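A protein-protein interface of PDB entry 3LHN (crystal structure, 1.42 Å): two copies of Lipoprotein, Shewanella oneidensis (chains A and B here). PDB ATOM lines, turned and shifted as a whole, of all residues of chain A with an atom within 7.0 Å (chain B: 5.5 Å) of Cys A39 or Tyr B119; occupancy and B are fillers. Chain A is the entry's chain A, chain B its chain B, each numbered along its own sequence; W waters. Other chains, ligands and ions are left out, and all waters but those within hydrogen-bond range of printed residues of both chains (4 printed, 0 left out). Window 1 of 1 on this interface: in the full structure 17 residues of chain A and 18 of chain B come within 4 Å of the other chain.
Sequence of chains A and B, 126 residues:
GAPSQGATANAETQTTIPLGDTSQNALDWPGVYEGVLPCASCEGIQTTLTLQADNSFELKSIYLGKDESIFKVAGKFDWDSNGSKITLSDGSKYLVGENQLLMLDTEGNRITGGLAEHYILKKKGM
Water W2 bridges the backbone carbonyl oxygen of Ala A40 (2.6 Å) and the backbone carbonyl oxygen of Pro B38 (2.8 Å). Water W4 bridges the backbone carbonyl oxygen of Ala B40 (2.7 Å) and the backbone carbonyl oxygen of Pro A38 (2.9 Å). Water W1 lies within hydrogen-bond range of the side-chain hydroxyl of Tyr B119 (2.8 Å), the backbone NH of Cys A39 (2.9 Å), the backbone carbonyl oxygen of Glu A43 (3.0 Å) and the backbone carbonyl oxygen of Cys A42 (3.3 Å). Water W3 bridges O of Glu A43 (2.9 Å) and N of Leu B115 (2.9 Å).
Hydrophobic or aromatic side chains of chain B within 4 Å of the printed part of chain A: Met B103, Ile B111, Leu B115 and Tyr B119. Among the printed residues, 12 pairs touch across the chains.
The side-chain hydroxyl (OH) of Tyr B119 lies within hydrogen-bond range of the backbone carbonyl oxygen (O) of Cys A39 (2.6 Å). The backbone carbonyl oxygen (O) of Cys A42 lies within hydrogen-bond range of the side-chain hydroxyl (OH) of Tyr B119.
Of the printed residues of chain B, Cys A39 touches Tyr B119 (2.6 Å). Of chain A, only Cys A39 (2.6 Å), Ala A40 (3.4 Å) and Cys A42 (3.1 Å) come within 4 Å of Tyr B119. Printed residues of chain A within 4 Å of Ile B111: Ser A41, Cys A42 and Glu A43. Of the printed residues of chain B, Glu A43 touches Ile B111. Of the printed residues of chain B, Pro A38 touches Ala B40 (3.99 Å). Printed residues of chain A within 4 Å of Ala B40: Pro A38 (3.99 Å) and Tyr A119 (3.5 Å). Ile B120 touches none of the printed residues of chain A.
N of Gly A44 lies close to SG of Cys A42, at 3.7 Å. The backbone NH (N) of Glu A43 is in hydrogen-bond range of the backbone carbonyl oxygen (O) of Leu A64, 3.3 Å away. N of Met B103 is in hydrogen-bond range of O of Tyr B119, at 2.9 Å. SG of Cys A39 forms a disulfide with SG of Cys A42 (2.1 Å).
Among the printed residues, merely in contact across the chains: Ala A40 with Met B103, Ala A40 with Tyr B119, Cys A42 with Ile B111, Tyr A119 with Ala B40, Ser A41 with Ile B111, Ser A41 with Met B103, Glu A43 with Ile B111, Leu A115 with Leu B115, Ala A40 with Pro B38 and Pro A38 with Ala B40.
Pro A38 touches Ala B40, and with the chains exchanged Ala A40 touches Pro B38. Ala A40 touches Tyr B119, and with the chains exchanged Tyr A119 touches Ala B40. Leu A115 touches its own counterpart, Leu B115.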
ATOM      1  N   VAL A  36       9.009  15.489 -11.885  1.00  0.00           N
ATOM      2  CA  VAL A  36       9.536  16.760 -11.420  1.00  0.00           C
ATOM      3  C   VAL A  36       9.081  16.920  -9.958  1.00  0.00           C
ATOM      4  O   VAL A  36       7.911  17.139  -9.680  1.00  0.00           O
ATOM      5  CB  VAL A  36       9.112  17.957 -12.245  1.00  0.00           C
ATOM      6  CG1 VAL A  36       9.813  19.240 -11.645  1.00  0.00           C
ATOM      7  CG2 VAL A  36       9.476  17.791 -13.749  1.00  0.00           C
ATOM      8  N   LEU A  37      10.005  16.721  -9.033  1.00  0.00           N
ATOM      9  CA  LEU A  37       9.718  16.682  -7.615  1.00  0.00           C
ATOM     10  C   LEU A  37       9.782  18.085  -7.041  1.00  0.00           C
ATOM     11  O   LEU A  37      10.495  18.963  -7.565  1.00  0.00           O
ATOM     12  CB  LEU A  37      10.766  15.827  -6.901  1.00  0.00           C
ATOM     13  CG  LEU A  37      10.854  14.320  -7.190  1.00  0.00           C
ATOM     14  CD1 LEU A  37      12.081  13.686  -6.577  1.00  0.00           C
ATOM     15  CD2 LEU A  37       9.602  13.599  -6.739  1.00  0.00           C
ATOM     16  N   PRO A  38       9.088  18.324  -5.921  1.00  0.00           N
ATOM     17  CA  PRO A  38       9.232  19.614  -5.279  1.00  0.00           C
ATOM     18  C   PRO A  38      10.617  19.840  -4.749  1.00  0.00           C
ATOM     19  O   PRO A  38      11.267  18.908  -4.300  1.00  0.00           O
ATOM     20  CB  PRO A  38       8.208  19.532  -4.110  1.00  0.00           C
ATOM     21  CG  PRO A  38       7.210  18.535  -4.592  1.00  0.00           C
ATOM     22  CD  PRO A  38       8.048  17.501  -5.269  1.00  0.00           C
ATOM     23  N   CYS A  39      11.042  21.102  -4.761  1.00  0.00           N
ATOM     24  CA  CYS A  39      12.401  21.469  -4.352  1.00  0.00           C
ATOM     25  C   CYS A  39      12.324  22.388  -3.153  1.00  0.00           C
ATOM     26  O   CYS A  39      11.552  23.318  -3.170  1.00  0.00           O
ATOM     27  CB  CYS A  39      13.061  22.170  -5.513  1.00  0.00           C
ATOM     28  SG  CYS A  39      14.805  22.583  -5.263  1.00  0.00           S
ATOM     29  N   ALA A  40      13.097  22.132  -2.106  1.00  0.00           N
ATOM     30  CA  ALA A  40      13.029  22.991  -0.918  1.00  0.00           C
ATOM     31  C   ALA A  40      13.325  24.458  -1.212  1.00  0.00           C
ATOM     32  O   ALA A  40      12.723  25.354  -0.603  1.00  0.00           O
ATOM     33  CB  ALA A  40      13.977  22.506   0.158  1.00  0.00           C
ATOM     34  N   SER A  41      14.236  24.725  -2.148  1.00  0.00           N
ATOM     35  CA  SER A  41      14.571  26.134  -2.422  1.00  0.00           C
ATOM     36  C   SER A  41      14.900  26.398  -3.868  1.00  0.00           C
ATOM     37  O   SER A  41      15.805  27.164  -4.189  1.00  0.00           O
ATOM     38  CB  SER A  41      15.726  26.614  -1.525  1.00  0.00           C
ATOM     39  OG  SER A  41      16.878  25.885  -1.838  1.00  0.00           O
ATOM     40  N   CYS A  42      14.082  25.838  -4.731  1.00  0.00           N
ATOM     41  CA  CYS A  42      14.242  26.024  -6.167  1.00  0.00           C
ATOM     42  C   CYS A  42      12.963  25.643  -6.863  1.00  0.00           C
ATOM     43  O   CYS A  42      12.018  25.161  -6.239  1.00  0.00           O
ATOM     44  CB  CYS A  42      15.457  25.263  -6.666  1.00  0.00           C
ATOM     45  SG  CYS A  42      15.273  23.528  -7.100  1.00  0.00           S
ATOM     46  N   GLU A  43      12.945  25.857  -8.169  1.00  0.00           N
ATOM     47  CA  GLU A  43      11.726  25.676  -8.929  1.00  0.00           C
ATOM     48  C   GLU A  43      11.183  24.253  -8.853  1.00  0.00           C
ATOM     49  O   GLU A  43       9.972  24.021  -8.804  1.00  0.00           O
ATOM     50  CB  GLU A  43      12.003  26.084 -10.383  1.00  0.00           C
ATOM     51  CG  GLU A  43      10.924  25.602 -11.335  1.00  0.00           C
ATOM     52  CD  GLU A  43      11.068  26.144 -12.729  1.00  0.00           C
ATOM     53  OE1 GLU A  43      11.656  27.225 -12.906  1.00  0.00           O
ATOM     54  OE2 GLU A  43      10.487  25.496 -13.613  1.00  0.00           O
ATOM     55  N   GLY A  44      12.066  23.253  -8.910  1.00  0.00           N
ATOM     56  CA  GLY A  44      11.652  21.886  -8.897  1.00  0.00           C
ATOM     57  C   GLY A  44      12.856  21.012  -9.239  1.00  0.00           C
ATOM     58  O   GLY A  44      13.892  21.541  -9.623  1.00  0.00           O
ATOM     59  N   ILE A  45      12.692  19.705  -9.107  1.00  0.00           N
ATOM     60  CA  ILE A  45      13.808  18.792  -9.341  1.00  0.00           C
ATOM     61  C   ILE A  45      13.406  17.834 -10.465  1.00  0.00           C
ATOM     62  O   ILE A  45      12.615  16.898 -10.226  1.00  0.00           O
ATOM     63  CB  ILE A  45      14.215  17.989  -8.121  1.00  0.00           C
ATOM     64  CG1 ILE A  45      14.313  18.851  -6.852  1.00  0.00           C
ATOM     65  CG2 ILE A  45      15.565  17.327  -8.386  1.00  0.00           C
ATOM     66  CD1 ILE A  45      14.530  18.019  -5.584  1.00  0.00           C
ATOM     67  N   TYR A  63      18.232  20.455 -10.730  1.00  0.00           N
ATOM     68  CA  TYR A  63      17.613  21.455  -9.890  1.00  0.00           C
ATOM     69  C   TYR A  63      17.337  22.671 -10.760  1.00  0.00           C
ATOM     70  O   TYR A  63      18.240  23.406 -11.164  1.00  0.00           O
ATOM     71  CB  TYR A  63      18.499  21.749  -8.688  1.00  0.00           C
ATOM     72  CG  TYR A  63      18.514  20.624  -7.702  1.00  0.00           C
ATOM     73  CD1 TYR A  63      19.297  19.485  -7.862  1.00  0.00           C
ATOM     74  CD2 TYR A  63      17.704  20.665  -6.589  1.00  0.00           C
ATOM     75  CE1 TYR A  63      19.246  18.426  -6.932  1.00  0.00           C
ATOM     76  CE2 TYR A  63      17.665  19.637  -5.679  1.00  0.00           C
ATOM     77  CZ  TYR A  63      18.428  18.523  -5.845  1.00  0.00           C
ATOM     78  OH  TYR A  63      18.346  17.513  -4.903  1.00  0.00           O
ATOM     79  N   LEU A  64      16.069  22.889 -11.030  1.00  0.00           N
ATOM     80  CA  LEU A  64      15.584  23.879 -11.977  1.00  0.00           C
ATOM     81  C   LEU A  64      15.576  25.269 -11.351  1.00  0.00           C
ATOM     82  O   LEU A  64      15.521  25.427 -10.132  1.00  0.00           O
ATOM     83  CB  LEU A  64      14.151  23.545 -12.398  1.00  0.00           C
ATOM     84  CG  LEU A  64      13.990  22.168 -13.019  1.00  0.00           C
ATOM     85  CD1 LEU A  64      12.490  21.877 -13.177  1.00  0.00           C
ATOM     86  CD2 LEU A  64      14.810  22.042 -14.339  1.00  0.00           C
ATOM     87  N   LEU A 115       0.668  18.852  -2.318  1.00  0.00           N
ATOM     88  CA  LEU A 115       1.599  18.476  -3.365  1.00  0.00           C
ATOM     89  C   LEU A 115       1.776  16.972  -3.504  1.00  0.00           C
ATOM     90  O   LEU A 115       2.725  16.545  -4.134  1.00  0.00           O
ATOM     91  CB  LEU A 115       2.960  19.150  -3.079  1.00  0.00           C
ATOM     92  CG  LEU A 115       2.949  20.683  -3.096  1.00  0.00           C
ATOM     93  CD1 LEU A 115       4.337  21.220  -2.846  1.00  0.00           C
ATOM     94  CD2 LEU A 115       2.399  21.290  -4.406  1.00  0.00           C
ATOM     95  N   TYR A 119       5.067  13.738  -6.050  1.00  0.00           N
ATOM     96  CA  TYR A 119       6.084  12.802  -5.587  1.00  0.00           C
ATOM     97  C   TYR A 119       6.106  11.500  -6.428  1.00  0.00           C
ATOM     98  O   TYR A 119       6.874  10.596  -6.153  1.00  0.00           O
ATOM     99  CB  TYR A 119       5.864  12.564  -4.068  1.00  0.00           C
ATOM    100  CG  TYR A 119       6.143  13.810  -3.303  1.00  0.00           C
ATOM    101  CD1 TYR A 119       7.429  14.193  -2.962  1.00  0.00           C
ATOM    102  CD2 TYR A 119       5.118  14.672  -2.963  1.00  0.00           C
ATOM    103  CE1 TYR A 119       7.686  15.365  -2.292  1.00  0.00           C
ATOM    104  CE2 TYR A 119       5.369  15.862  -2.323  1.00  0.00           C
ATOM    105  CZ  TYR A 119       6.655  16.207  -1.986  1.00  0.00           C
ATOM    106  OH  TYR A 119       6.884  17.418  -1.347  1.00  0.00           O
ATOM    107  N   LEU B  37       5.954  25.747   3.369  1.00  0.00           N
ATOM    108  CA  LEU B  37       6.875  25.723   2.265  1.00  0.00           C
ATOM    109  C   LEU B  37       6.963  24.305   1.688  1.00  0.00           C
ATOM    110  O   LEU B  37       6.716  23.305   2.393  1.00  0.00           O
ATOM    111  CB  LEU B  37       8.288  26.090   2.728  1.00  0.00           C
ATOM    112  CG  LEU B  37       8.508  27.501   3.297  1.00  0.00           C
ATOM    113  CD1 LEU B  37       9.914  27.586   3.955  1.00  0.00           C
ATOM    114  CD2 LEU B  37       8.373  28.499   2.194  1.00  0.00           C
ATOM    115  N   PRO B  38       7.316  24.161   0.411  1.00  0.00           N
ATOM    116  CA  PRO B  38       7.520  22.814  -0.132  1.00  0.00           C
ATOM    117  C   PRO B  38       8.650  22.092   0.567  1.00  0.00           C
ATOM    118  O   PRO B  38       9.661  22.682   0.906  1.00  0.00           O
ATOM    119  CB  PRO B  38       7.873  23.074  -1.600  1.00  0.00           C
ATOM    120  CG  PRO B  38       7.197  24.375  -1.906  1.00  0.00           C
ATOM    121  CD  PRO B  38       7.415  25.188  -0.624  1.00  0.00           C
ATOM    122  N   ALA B  40      11.266  18.699   0.406  1.00  0.00           N
ATOM    123  CA  ALA B  40      11.837  17.729  -0.533  1.00  0.00           C
ATOM    124  C   ALA B  40      11.273  16.338  -0.330  1.00  0.00           C
ATOM    125  O   ALA B  40      11.077  15.608  -1.291  1.00  0.00           O
ATOM    126  CB  ALA B  40      13.400  17.732  -0.487  1.00  0.00           C
ATOM    127  N   LEU B 101       7.657  37.774   3.573  1.00  0.00           N
ATOM    128  CA  LEU B 101       9.021  37.424   3.212  1.00  0.00           C
ATOM    129  C   LEU B 101       8.881  36.402   2.077  1.00  0.00           C
ATOM    130  O   LEU B 101       7.975  35.560   2.124  1.00  0.00           O
ATOM    131  CB  LEU B 101       9.761  36.779   4.364  1.00  0.00           C
ATOM    132  CG  LEU B 101       9.879  37.598   5.656  1.00  0.00           C
ATOM    133  CD1 LEU B 101      10.631  36.764   6.716  1.00  0.00           C
ATOM    134  CD2 LEU B 101      10.608  38.903   5.417  1.00  0.00           C
ATOM    135  N   LEU B 102       9.774  36.433   1.120  1.00  0.00           N
ATOM    136  CA  LEU B 102       9.722  35.512  -0.017  1.00  0.00           C
ATOM    137  C   LEU B 102      11.010  34.752   0.032  1.00  0.00           C
ATOM    138  O   LEU B 102      12.085  35.357  -0.105  1.00  0.00           O
ATOM    139  CB  LEU B 102       9.578  36.282  -1.320  1.00  0.00           C
ATOM    140  CG  LEU B 102       9.698  35.409  -2.575  1.00  0.00           C
ATOM    141  CD1 LEU B 102       8.499  34.376  -2.637  1.00  0.00           C
ATOM    142  CD2 LEU B 102       9.722  36.259  -3.860  1.00  0.00           C
ATOM    143  N   MET B 103      10.951  33.445   0.253  1.00  0.00           N
ATOM    144  CA  MET B 103      12.197  32.698   0.330  1.00  0.00           C
ATOM    145  C   MET B 103      12.791  32.539  -1.071  1.00  0.00           C
ATOM    146  O   MET B 103      12.095  32.171  -2.022  1.00  0.00           O
ATOM    147  CB  MET B 103      12.041  31.339   0.983  1.00  0.00           C
ATOM    148  CG  MET B 103      13.377  30.833   1.520  1.00  0.00           C
ATOM    149  SD  MET B 103      13.329  29.102   2.340  1.00  0.00           S
ATOM    150  CE  MET B 103      13.253  28.274   0.565  1.00  0.00           C
ATOM    151  N   ILE B 111      12.540  32.232  -6.890  1.00  0.00           N
ATOM    152  CA  ILE B 111      12.172  30.878  -7.267  1.00  0.00           C
ATOM    153  C   ILE B 111      10.994  30.977  -8.222  1.00  0.00           C
ATOM    154  O   ILE B 111       9.959  31.573  -7.890  1.00  0.00           O
ATOM    155  CB  ILE B 111      11.871  30.043  -6.016  1.00  0.00           C
ATOM    156  CG1 ILE B 111      13.144  29.936  -5.166  1.00  0.00           C
ATOM    157  CG2 ILE B 111      11.356  28.633  -6.418  1.00  0.00           C
ATOM    158  CD1 ILE B 111      12.892  29.331  -3.753  1.00  0.00           C
ATOM    159  N   LEU B 115       5.173  26.452  -8.622  1.00  0.00           N
ATOM    160  CA  LEU B 115       5.011  26.535  -7.177  1.00  0.00           C
ATOM    161  C   LEU B 115       5.581  27.831  -6.584  1.00  0.00           C
ATOM    162  O   LEU B 115       5.764  27.934  -5.391  1.00  0.00           O
ATOM    163  CB  LEU B 115       5.657  25.325  -6.490  1.00  0.00           C
ATOM    164  CG  LEU B 115       5.131  23.950  -6.927  1.00  0.00           C
ATOM    165  CD1 LEU B 115       5.850  22.861  -6.096  1.00  0.00           C
ATOM    166  CD2 LEU B 115       3.607  23.801  -6.760  1.00  0.00           C
ATOM    167  N   ALA B 116       5.841  28.833  -7.431  1.00  0.00           N
ATOM    168  CA  ALA B 116       6.489  30.061  -6.965  1.00  0.00           C
ATOM    169  C   ALA B 116       5.821  30.682  -5.749  1.00  0.00           C
ATOM    170  O   ALA B 116       6.497  31.207  -4.863  1.00  0.00           O
ATOM    171  CB  ALA B 116       6.525  31.128  -8.089  1.00  0.00           C
ATOM    172  N   GLU B 117       4.497  30.664  -5.701  1.00  0.00           N
ATOM    173  CA  GLU B 117       3.810  31.301  -4.561  1.00  0.00           C
ATOM    174  C   GLU B 117       3.903  30.544  -3.265  1.00  0.00           C
ATOM    175  O   GLU B 117       3.642  31.100  -2.183  1.00  0.00           O
ATOM    176  CB  GLU B 117       2.331  31.550  -4.899  1.00  0.00           C
ATOM    177  CG  GLU B 117       2.157  32.533  -6.059  1.00  0.00           C
ATOM    178  CD  GLU B 117       2.248  33.967  -5.605  1.00  0.00           C
ATOM    179  OE1 GLU B 117       1.328  34.439  -4.875  1.00  0.00           O
ATOM    180  OE2 GLU B 117       3.223  34.635  -5.976  1.00  0.00           O
ATOM    181  N   HIS B 118       4.302  29.275  -3.341  1.00  0.00           N
ATOM    182  CA  HIS B 118       4.450  28.488  -2.117  1.00  0.00           C
ATOM    183  C   HIS B 118       5.644  28.900  -1.281  1.00  0.00           C
ATOM    184  O   HIS B 118       5.815  28.360  -0.203  1.00  0.00           O
ATOM    185  CB  HIS B 118       4.593  27.020  -2.472  1.00  0.00           C
ATOM    186  CG  HIS B 118       3.340  26.415  -3.023  1.00  0.00           C
ATOM    187  ND1 HIS B 118       2.683  25.403  -2.370  1.00  0.00           N
ATOM    188  CD2 HIS B 118       2.642  26.658  -4.156  1.00  0.00           C
ATOM    189  CE1 HIS B 118       1.604  25.063  -3.069  1.00  0.00           C
ATOM    190  NE2 HIS B 118       1.551  25.809  -4.152  1.00  0.00           N
ATOM    191  N   TYR B 119       6.486  29.799  -1.779  1.00  0.00           N
ATOM    192  CA  TYR B 119       7.703  30.215  -1.087  1.00  0.00           C
ATOM    193  C   TYR B 119       7.474  31.520  -0.291  1.00  0.00           C
ATOM    194  O   TYR B 119       8.400  32.080   0.301  1.00  0.00           O
ATOM    195  CB  TYR B 119       8.884  30.304  -2.080  1.00  0.00           C
ATOM    196  CG  TYR B 119       9.173  28.949  -2.603  1.00  0.00           C
ATOM    197  CD1 TYR B 119       9.994  28.045  -1.912  1.00  0.00           C
ATOM    198  CD2 TYR B 119       8.595  28.528  -3.776  1.00  0.00           C
ATOM    199  CE1 TYR B 119      10.231  26.789  -2.408  1.00  0.00           C
ATOM    200  CE2 TYR B 119       8.789  27.246  -4.269  1.00  0.00           C
ATOM    201  CZ  TYR B 119       9.596  26.366  -3.580  1.00  0.00           C
ATOM    202  OH  TYR B 119       9.782  25.049  -4.072  1.00  0.00           O
ATOM    203  N   ILE B 120       6.231  31.988  -0.237  1.00  0.00           N
ATOM    204  CA  ILE B 120       5.872  33.206   0.520  1.00  0.00           C
ATOM    205  C   ILE B 120       5.544  32.885   1.983  1.00  0.00           C
ATOM    206  O   ILE B 120       4.805  31.935   2.252  1.00  0.00           O
ATOM    207  CB  ILE B 120       4.664  33.899  -0.087  1.00  0.00           C
ATOM    208  CG1 ILE B 120       4.986  34.421  -1.497  1.00  0.00           C
ATOM    209  CG2 ILE B 120       4.140  35.084   0.795  1.00  0.00           C
ATOM    210  CD1 ILE B 120       3.777  34.866  -2.348  1.00  0.00           C
ATOM    211  N   LEU B 121       6.103  33.662   2.893  1.00  0.00           N
ATOM    212  CA  LEU B 121       5.753  33.617   4.330  1.00  0.00           C
ATOM    213  C   LEU B 121       5.048  34.934   4.593  1.00  0.00           C
ATOM    214  O   LEU B 121       5.665  35.979   4.495  1.00  0.00           O
ATOM    215  CB  LEU B 121       6.978  33.455   5.226  1.00  0.00           C
ATOM    216  CG  LEU B 121       7.900  32.270   4.964  1.00  0.00           C
ATOM    217  CD1 LEU B 121       9.039  32.248   5.967  1.00  0.00           C
ATOM    218  CD2 LEU B 121       7.162  30.971   5.020  1.00  0.00           C
HETATM  219  O   HOH W   1       9.410  23.072  -6.055  1.00  0.00           O
HETATM  220  O   HOH W   2      11.288  24.868   1.570  1.00  0.00           O
HETATM  221  O   HOH W   3       8.053  26.175  -8.857  1.00  0.00           O
HETATM  222  O   HOH W   4      12.032  16.189  -3.716  1.00  0.00           O
